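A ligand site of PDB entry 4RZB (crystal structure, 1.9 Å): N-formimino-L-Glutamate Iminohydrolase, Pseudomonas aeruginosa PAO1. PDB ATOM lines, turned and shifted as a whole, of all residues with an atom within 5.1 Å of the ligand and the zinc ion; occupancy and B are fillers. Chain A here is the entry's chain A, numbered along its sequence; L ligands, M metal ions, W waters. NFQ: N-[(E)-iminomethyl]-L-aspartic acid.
An oxygen (O2) of the ligand sits at hydrogen-bond distance from a ring nitrogen (NE2) of His 206 (2.7 Å).
An oxygen (OD2) of the ligand is in salt-bridge range of the guanidinium group of Arg 82, 3.1 Å away.
OD2 of Asp 320 is in salt-bridge range of NF of the ligand (3.7 Å).
An oxygen (O1) of the ligand lies within hydrogen-bond range of the side-chain hydroxyl (OH) of Tyr 121 (2.6 Å).
NE2 of Gln 61 sits at hydrogen-bond distance from O1 of the ligand.
The guanidinium group (NH2) of Arg 209 lies within salt-bridge range of an oxygen (OD1) of the ligand (2.9 Å).
A nitrogen (NF) of the ligand lies within salt-bridge range of the side-chain carboxylate of Glu 235 (3.0 Å).
OH of Tyr 121 sits at hydrogen-bond distance from NE2 of Gln 61 (2.8 Å).
A ring nitrogen (ND1) of His 232 sits at hydrogen-bond distance from the backbone carbonyl oxygen of His 206 (2.9 Å).
The side-chain carboxylate (OE1) of Glu 235 sits close to a ring nitrogen (NE2) of His 269 (3.4 Å).
NH1 of Arg 82 lies close to OH of Tyr 86 (3.2 Å).
Merely in contact with the ligand: Leu 298, Phe 78, Trp 81 and Met 85.
Within 4 Å of the ligand: His 58, Gln 61, Phe 78, Trp 81, Arg 82, Met 85, Tyr 121, His 206, Arg 209, His 232, Glu 235, Leu 298 and Asp 320.
The nearest printed residue that does not touch the ligand is His 269 (4.2 Å).
The nearest printed residue that does not touch the zinc ion is His 269 (4.02 Å).
The zinc ion is bound by water W4 (2.0 Å), a ring nitrogen (NE2) of His 58 (2.0 Å), a ring nitrogen (NE2) of His 56 (2.0 Å), a ring nitrogen (NE2) of His 232 (2.2 Å) and the side-chain carboxylate of Asp 320 (2.5 Å).
Water W4 lies within hydrogen-bond range of the side-chain carboxylate (OD2) of Asp 320, a ring nitrogen (NE2) of His 269 and a nitrogen (NF) of the ligand.
Water W2 lies within hydrogen-bond range of an oxygen (O2) of the ligand (2.7 Å) and the side-chain hydroxyl (OH) of Tyr 121 (3.5 Å).
Water W3 lies within hydrogen-bond range of OH of Tyr 86 (2.7 Å), OH of Tyr 159 (2.7 Å), OD2 of the ligand (2.8 Å) and NH1 of Arg 82 (3.4 Å).
Water W1 lies within hydrogen-bond range of a nitrogen (NF) of the ligand (2.9 Å) and the side-chain amide oxygen of Gln 61 (3.0 Å).
Water W5 lies within hydrogen-bond range of OE1 of Glu 235 (2.5 Å), OD1 of the ligand (2.9 Å) and NH2 of Arg 209 (3.2 Å).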
ATOM      1  N   HIS A  56       7.309  22.227   4.051  1.00  0.00           N
ATOM      2  CA  HIS A  56       8.215  21.430   4.898  1.00  0.00           C
ATOM      3  C   HIS A  56       7.477  20.751   6.045  1.00  0.00           C
ATOM      4  O   HIS A  56       6.904  21.431   6.900  1.00  0.00           O
ATOM      5  CB  HIS A  56       9.359  22.305   5.444  1.00  0.00           C
ATOM      6  CG  HIS A  56      10.436  21.525   6.142  1.00  0.00           C
ATOM      7  ND1 HIS A  56      11.293  20.671   5.462  1.00  0.00           N
ATOM      8  CD2 HIS A  56      10.805  21.470   7.443  1.00  0.00           C
ATOM      9  CE1 HIS A  56      12.137  20.131   6.327  1.00  0.00           C
ATOM     10  NE2 HIS A  56      11.866  20.594   7.530  1.00  0.00           N
ATOM     11  N   HIS A  58       7.660  17.044   8.767  1.00  0.00           N
ATOM     12  CA  HIS A  58       8.007  15.690   9.224  1.00  0.00           C
ATOM     13  C   HIS A  58       6.827  15.130   9.988  1.00  0.00           C
ATOM     14  O   HIS A  58       6.692  15.386  11.197  1.00  0.00           O
ATOM     15  CB  HIS A  58       9.243  15.674  10.124  1.00  0.00           C
ATOM     16  CG  HIS A  58      10.369  16.530   9.635  1.00  0.00           C
ATOM     17  ND1 HIS A  58      11.011  16.308   8.430  1.00  0.00           N
ATOM     18  CD2 HIS A  58      10.995  17.595  10.197  1.00  0.00           C
ATOM     19  CE1 HIS A  58      11.969  17.201   8.278  1.00  0.00           C
ATOM     20  NE2 HIS A  58      11.978  17.995   9.325  1.00  0.00           N
ATOM     21  N   GLN A  61       6.250  13.874  13.745  1.00  0.00           N
ATOM     22  CA  GLN A  61       6.577  14.752  14.855  1.00  0.00           C
ATOM     23  C   GLN A  61       5.330  15.371  15.491  1.00  0.00           C
ATOM     24  O   GLN A  61       5.348  15.787  16.649  1.00  0.00           O
ATOM     25  CB  GLN A  61       7.587  15.823  14.424  1.00  0.00           C
ATOM     26  CG  GLN A  61       8.980  15.218  14.157  1.00  0.00           C
ATOM     27  CD  GLN A  61      10.039  16.248  13.814  1.00  0.00           C
ATOM     28  OE1 GLN A  61       9.825  17.453  13.987  1.00  0.00           O
ATOM     29  NE2 GLN A  61      11.198  15.780  13.315  1.00  0.00           N
ATOM     30  N   PHE A  78      18.186  22.793  21.319  1.00  0.00           N
ATOM     31  CA  PHE A  78      17.799  22.084  20.120  1.00  0.00           C
ATOM     32  C   PHE A  78      18.275  20.623  20.193  1.00  0.00           C
ATOM     33  O   PHE A  78      17.563  19.710  19.804  1.00  0.00           O
ATOM     34  CB  PHE A  78      18.420  22.813  18.926  1.00  0.00           C
ATOM     35  CG  PHE A  78      18.234  22.116  17.617  1.00  0.00           C
ATOM     36  CD1 PHE A  78      17.184  22.450  16.784  1.00  0.00           C
ATOM     37  CD2 PHE A  78      19.143  21.147  17.209  1.00  0.00           C
ATOM     38  CE1 PHE A  78      17.019  21.814  15.582  1.00  0.00           C
ATOM     39  CE2 PHE A  78      18.982  20.506  15.998  1.00  0.00           C
ATOM     40  CZ  PHE A  78      17.922  20.837  15.188  1.00  0.00           C
ATOM     41  N   TRP A  79      19.484  20.411  20.722  1.00  0.00           N
ATOM     42  CA  TRP A  79      20.062  19.074  20.696  1.00  0.00           C
ATOM     43  C   TRP A  79      19.424  18.113  21.684  1.00  0.00           C
ATOM     44  O   TRP A  79      19.288  16.925  21.395  1.00  0.00           O
ATOM     45  CB  TRP A  79      21.599  19.150  20.824  1.00  0.00           C
ATOM     46  CG  TRP A  79      22.122  20.095  19.800  1.00  0.00           C
ATOM     47  CD1 TRP A  79      22.515  21.388  19.998  1.00  0.00           C
ATOM     48  CD2 TRP A  79      22.221  19.856  18.390  1.00  0.00           C
ATOM     49  NE1 TRP A  79      22.892  21.956  18.799  1.00  0.00           N
ATOM     50  CE2 TRP A  79      22.717  21.038  17.803  1.00  0.00           C
ATOM     51  CE3 TRP A  79      21.959  18.750  17.569  1.00  0.00           C
ATOM     52  CZ2 TRP A  79      22.959  21.154  16.436  1.00  0.00           C
ATOM     53  CZ3 TRP A  79      22.190  18.864  16.210  1.00  0.00           C
ATOM     54  CH2 TRP A  79      22.690  20.059  15.654  1.00  0.00           C
ATOM     55  N   TRP A  81      16.278  18.492  22.609  1.00  0.00           N
ATOM     56  CA  TRP A  81      14.986  18.253  21.955  1.00  0.00           C
ATOM     57  C   TRP A  81      15.142  17.139  20.936  1.00  0.00           C
ATOM     58  O   TRP A  81      14.302  16.242  20.838  1.00  0.00           O
ATOM     59  CB  TRP A  81      14.466  19.506  21.237  1.00  0.00           C
ATOM     60  CG  TRP A  81      13.325  19.201  20.246  1.00  0.00           C
ATOM     61  CD1 TRP A  81      11.999  19.139  20.534  1.00  0.00           C
ATOM     62  CD2 TRP A  81      13.449  18.915  18.846  1.00  0.00           C
ATOM     63  NE1 TRP A  81      11.274  18.831  19.390  1.00  0.00           N
ATOM     64  CE2 TRP A  81      12.143  18.687  18.348  1.00  0.00           C
ATOM     65  CE3 TRP A  81      14.532  18.830  17.959  1.00  0.00           C
ATOM     66  CZ2 TRP A  81      11.901  18.384  17.011  1.00  0.00           C
ATOM     67  CZ3 TRP A  81      14.283  18.521  16.623  1.00  0.00           C
ATOM     68  CH2 TRP A  81      12.982  18.304  16.169  1.00  0.00           C
ATOM     69  N   ARG A  82      16.232  17.197  20.156  1.00  0.00           N
ATOM     70  CA  ARG A  82      16.412  16.226  19.082  1.00  0.00           C
ATOM     71  C   ARG A  82      16.531  14.794  19.614  1.00  0.00           C
ATOM     72  O   ARG A  82      16.031  13.855  18.985  1.00  0.00           O
ATOM     73  CB  ARG A  82      17.619  16.584  18.197  1.00  0.00           C
ATOM     74  CG  ARG A  82      17.566  15.894  16.839  1.00  0.00           C
ATOM     75  CD  ARG A  82      18.795  16.160  15.988  1.00  0.00           C
ATOM     76  NE  ARG A  82      20.017  15.559  16.538  1.00  0.00           N
ATOM     77  CZ  ARG A  82      21.126  15.372  15.835  1.00  0.00           C
ATOM     78  NH1 ARG A  82      21.156  15.747  14.561  1.00  0.00           N
ATOM     79  NH2 ARG A  82      22.202  14.811  16.392  1.00  0.00           N
ATOM     80  N   MET A  85      13.076  13.546  20.301  1.00  0.00           N
ATOM     81  CA  MET A  85      12.477  13.230  19.004  1.00  0.00           C
ATOM     82  C   MET A  85      12.960  11.874  18.499  1.00  0.00           C
ATOM     83  O   MET A  85      12.183  11.068  17.969  1.00  0.00           O
ATOM     84  CB  MET A  85      12.829  14.329  18.002  1.00  0.00           C
ATOM     85  CG  MET A  85      12.139  14.189  16.637  1.00  0.00           C
ATOM     86  SD  MET A  85      13.078  13.217  15.442  1.00  0.00           S
ATOM     87  CE  MET A  85      14.397  14.383  15.040  1.00  0.00           C
ATOM     88  N   TYR A  86      14.255  11.612  18.681  1.00  0.00           N
ATOM     89  CA  TYR A  86      14.833  10.322  18.307  1.00  0.00           C
ATOM     90  C   TYR A  86      14.168   9.171  19.077  1.00  0.00           C
ATOM     91  O   TYR A  86      13.919   8.096  18.519  1.00  0.00           O
ATOM     92  CB  TYR A  86      16.354  10.310  18.548  1.00  0.00           C
ATOM     93  CG  TYR A  86      17.195  11.026  17.491  1.00  0.00           C
ATOM     94  CD1 TYR A  86      16.618  11.700  16.415  1.00  0.00           C
ATOM     95  CD2 TYR A  86      18.590  11.005  17.570  1.00  0.00           C
ATOM     96  CE1 TYR A  86      17.407  12.341  15.450  1.00  0.00           C
ATOM     97  CE2 TYR A  86      19.367  11.630  16.633  1.00  0.00           C
ATOM     98  CZ  TYR A  86      18.797  12.296  15.577  1.00  0.00           C
ATOM     99  OH  TYR A  86      19.634  12.896  14.663  1.00  0.00           O
ATOM    100  N   TYR A 121      12.312  11.094   6.241  1.00  0.00           N
ATOM    101  CA  TYR A 121      13.563  10.376   6.495  1.00  0.00           C
ATOM    102  C   TYR A 121      13.425   9.109   7.345  1.00  0.00           C
ATOM    103  O   TYR A 121      14.421   8.475   7.672  1.00  0.00           O
ATOM    104  CB  TYR A 121      14.605  11.304   7.129  1.00  0.00           C
ATOM    105  CG  TYR A 121      14.136  12.067   8.350  1.00  0.00           C
ATOM    106  CD1 TYR A 121      13.908  11.421   9.550  1.00  0.00           C
ATOM    107  CD2 TYR A 121      13.940  13.448   8.293  1.00  0.00           C
ATOM    108  CE1 TYR A 121      13.487  12.135  10.683  1.00  0.00           C
ATOM    109  CE2 TYR A 121      13.533  14.158   9.408  1.00  0.00           C
ATOM    110  CZ  TYR A 121      13.303  13.498  10.593  1.00  0.00           C
ATOM    111  OH  TYR A 121      12.915  14.216  11.700  1.00  0.00           O
ATOM    112  N   TYR A 159      20.122  10.298   4.108  1.00  0.00           N
ATOM    113  CA  TYR A 159      20.655  10.505   5.450  1.00  0.00           C
ATOM    114  C   TYR A 159      21.672   9.403   5.677  1.00  0.00           C
ATOM    115  O   TYR A 159      21.322   8.223   5.590  1.00  0.00           O
ATOM    116  CB  TYR A 159      19.537  10.401   6.495  1.00  0.00           C
ATOM    117  CG  TYR A 159      19.846  11.039   7.834  1.00  0.00           C
ATOM    118  CD1 TYR A 159      19.023  12.035   8.356  1.00  0.00           C
ATOM    119  CD2 TYR A 159      20.965  10.661   8.584  1.00  0.00           C
ATOM    120  CE1 TYR A 159      19.295  12.632   9.571  1.00  0.00           C
ATOM    121  CE2 TYR A 159      21.248  11.262   9.813  1.00  0.00           C
ATOM    122  CZ  TYR A 159      20.416  12.252  10.300  1.00  0.00           C
ATOM    123  OH  TYR A 159      20.666  12.860  11.513  1.00  0.00           O
ATOM    124  N   HIS A 206      19.295  15.418   3.864  1.00  0.00           N
ATOM    125  CA  HIS A 206      18.842  15.874   5.182  1.00  0.00           C
ATOM    126  C   HIS A 206      19.477  17.210   5.579  1.00  0.00           C
ATOM    127  O   HIS A 206      18.778  18.124   6.012  1.00  0.00           O
ATOM    128  CB  HIS A 206      19.100  14.847   6.279  1.00  0.00           C
ATOM    129  CG  HIS A 206      18.743  15.363   7.648  1.00  0.00           C
ATOM    130  ND1 HIS A 206      19.651  16.003   8.458  1.00  0.00           N
ATOM    131  CD2 HIS A 206      17.567  15.360   8.319  1.00  0.00           C
ATOM    132  CE1 HIS A 206      19.056  16.355   9.587  1.00  0.00           C
ATOM    133  NE2 HIS A 206      17.796  15.980   9.531  1.00  0.00           N
ATOM    134  N   ARG A 209      25.317  18.071   7.589  1.00  0.00           N
ATOM    135  CA  ARG A 209      25.830  17.220   8.664  1.00  0.00           C
ATOM    136  C   ARG A 209      25.649  15.746   8.319  1.00  0.00           C
ATOM    137  O   ARG A 209      26.441  14.891   8.712  1.00  0.00           O
ATOM    138  CB  ARG A 209      25.083  17.516   9.969  1.00  0.00           C
ATOM    139  CG  ARG A 209      25.494  18.815  10.671  1.00  0.00           C
ATOM    140  CD  ARG A 209      24.441  19.210  11.714  1.00  0.00           C
ATOM    141  NE  ARG A 209      23.192  19.712  11.111  1.00  0.00           N
ATOM    142  CZ  ARG A 209      21.993  19.157  11.257  1.00  0.00           C
ATOM    143  NH1 ARG A 209      21.824  18.053  11.984  1.00  0.00           N
ATOM    144  NH2 ARG A 209      20.935  19.710  10.674  1.00  0.00           N
ATOM    145  N   HIS A 232      17.836  20.804   4.722  1.00  0.00           N
ATOM    146  CA  HIS A 232      17.907  21.642   5.925  1.00  0.00           C
ATOM    147  C   HIS A 232      19.249  22.344   5.886  1.00  0.00           C
ATOM    148  O   HIS A 232      20.280  21.685   5.691  1.00  0.00           O
ATOM    149  CB  HIS A 232      17.941  20.830   7.241  1.00  0.00           C
ATOM    150  CG  HIS A 232      16.657  20.154   7.622  1.00  0.00           C
ATOM    151  ND1 HIS A 232      16.578  18.792   7.805  1.00  0.00           N
ATOM    152  CD2 HIS A 232      15.444  20.647   7.944  1.00  0.00           C
ATOM    153  CE1 HIS A 232      15.358  18.470   8.176  1.00  0.00           C
ATOM    154  NE2 HIS A 232      14.642  19.581   8.271  1.00  0.00           N
ATOM    155  N   GLU A 235      20.294  26.006  10.232  1.00  0.00           N
ATOM    156  CA  GLU A 235      19.262  26.195  11.248  1.00  0.00           C
ATOM    157  C   GLU A 235      19.839  26.624  12.608  1.00  0.00           C
ATOM    158  O   GLU A 235      19.287  27.509  13.266  1.00  0.00           O
ATOM    159  CB  GLU A 235      18.426  24.937  11.415  1.00  0.00           C
ATOM    160  CG  GLU A 235      17.284  25.118  12.419  1.00  0.00           C
ATOM    161  CD  GLU A 235      16.428  23.886  12.600  1.00  0.00           C
ATOM    162  OE1 GLU A 235      16.822  22.792  12.125  1.00  0.00           O
ATOM    163  OE2 GLU A 235      15.344  23.991  13.236  1.00  0.00           O
ATOM    164  N   VAL A 268      15.805  24.892   3.528  1.00  0.00           N
ATOM    165  CA  VAL A 268      14.934  24.951   4.710  1.00  0.00           C
ATOM    166  C   VAL A 268      15.653  25.593   5.890  1.00  0.00           C
ATOM    167  O   VAL A 268      16.804  25.261   6.187  1.00  0.00           O
ATOM    168  CB  VAL A 268      14.403  23.559   5.098  1.00  0.00           C
ATOM    169  CG1 VAL A 268      13.322  23.684   6.178  1.00  0.00           C
ATOM    170  CG2 VAL A 268      13.811  22.849   3.859  1.00  0.00           C
ATOM    171  N   HIS A 269      14.934  26.513   6.551  1.00  0.00           N
ATOM    172  CA  HIS A 269      15.402  27.371   7.629  1.00  0.00           C
ATOM    173  C   HIS A 269      16.306  28.491   7.120  1.00  0.00           C
ATOM    174  O   HIS A 269      15.892  29.665   7.104  1.00  0.00           O
ATOM    175  CB  HIS A 269      16.066  26.574   8.767  1.00  0.00           C
ATOM    176  CG  HIS A 269      15.227  25.435   9.262  1.00  0.00           C
ATOM    177  ND1 HIS A 269      13.941  25.610   9.739  1.00  0.00           N
ATOM    178  CD2 HIS A 269      15.473  24.104   9.311  1.00  0.00           C
ATOM    179  CE1 HIS A 269      13.450  24.440  10.095  1.00  0.00           C
ATOM    180  NE2 HIS A 269      14.352  23.505   9.844  1.00  0.00           N
ATOM    181  N   THR A 294       8.053  26.501  14.401  1.00  0.00           N
ATOM    182  CA  THR A 294       9.063  25.531  14.829  1.00  0.00           C
ATOM    183  C   THR A 294      10.397  26.202  15.185  1.00  0.00           C
ATOM    184  O   THR A 294      11.026  25.863  16.185  1.00  0.00           O
ATOM    185  CB  THR A 294       9.269  24.400  13.778  1.00  0.00           C
ATOM    186  OG1 THR A 294       8.117  23.534  13.785  1.00  0.00           O
ATOM    187  CG2 THR A 294      10.503  23.562  14.125  1.00  0.00           C
ATOM    188  N   LEU A 298      12.055  25.883  18.766  1.00  0.00           N
ATOM    189  CA  LEU A 298      13.362  25.266  18.939  1.00  0.00           C
ATOM    190  C   LEU A 298      14.463  26.281  19.287  1.00  0.00           C
ATOM    191  O   LEU A 298      15.639  25.899  19.500  1.00  0.00           O
ATOM    192  CB  LEU A 298      13.726  24.457  17.692  1.00  0.00           C
ATOM    193  CG  LEU A 298      12.781  23.279  17.418  1.00  0.00           C
ATOM    194  CD1 LEU A 298      13.224  22.514  16.165  1.00  0.00           C
ATOM    195  CD2 LEU A 298      12.730  22.360  18.616  1.00  0.00           C
ATOM    196  N   ASP A 320       6.764  21.973   9.613  1.00  0.00           N
ATOM    197  CA  ASP A 320       7.987  21.306  10.139  1.00  0.00           C
ATOM    198  C   ASP A 320       7.738  20.279  11.273  1.00  0.00           C
ATOM    199  O   ASP A 320       7.354  19.149  11.003  1.00  0.00           O
ATOM    200  CB  ASP A 320       9.039  22.355  10.558  1.00  0.00           C
ATOM    201  CG  ASP A 320      10.412  21.755  10.795  1.00  0.00           C
ATOM    202  OD1 ASP A 320      10.598  20.547  10.517  1.00  0.00           O
ATOM    203  OD2 ASP A 320      11.312  22.482  11.257  1.00  0.00           O
HETATM  204  C   NFQ L   1      14.960  16.899  11.787  1.00  0.00           C
HETATM  205  N   NFQ L   1      14.597  19.007  12.832  1.00  0.00           N
HETATM  206  O1  NFQ L   1      13.743  16.683  12.079  1.00  0.00           O
HETATM  207  O2  NFQ L   1      15.614  16.015  11.178  1.00  0.00           O
HETATM  208  CA  NFQ L   1      15.599  18.196  12.171  1.00  0.00           C
HETATM  209  CB  NFQ L   1      16.765  17.930  13.082  1.00  0.00           C
HETATM  210  CF  NFQ L   1      15.031  20.357  12.967  1.00  0.00           C
HETATM  211  NF  NFQ L   1      14.126  21.238  13.340  1.00  0.00           N
HETATM  212  CG  NFQ L   1      18.116  17.956  12.451  1.00  0.00           C
HETATM  213  OD1 NFQ L   1      18.357  18.797  11.545  1.00  0.00           O
HETATM  214  OD2 NFQ L   1      19.004  17.138  12.813  1.00  0.00           O
HETATM  215 ZN    ZN M   1      12.705  19.883   9.260  1.00  0.00          ZN
HETATM  216  O   HOH W   1      11.769  19.563  13.160  1.00  0.00           O
HETATM  217  O   HOH W   2      16.299  13.531  11.850  1.00  0.00           O
HETATM  218  O   HOH W   3      18.699  14.359  12.652  1.00  0.00           O
HETATM  219  O   HOH W   4      13.425  21.211  10.540  1.00  0.00           O
HETATM  220  O   HOH W   5      18.365  21.546  10.526  1.00  0.00           O
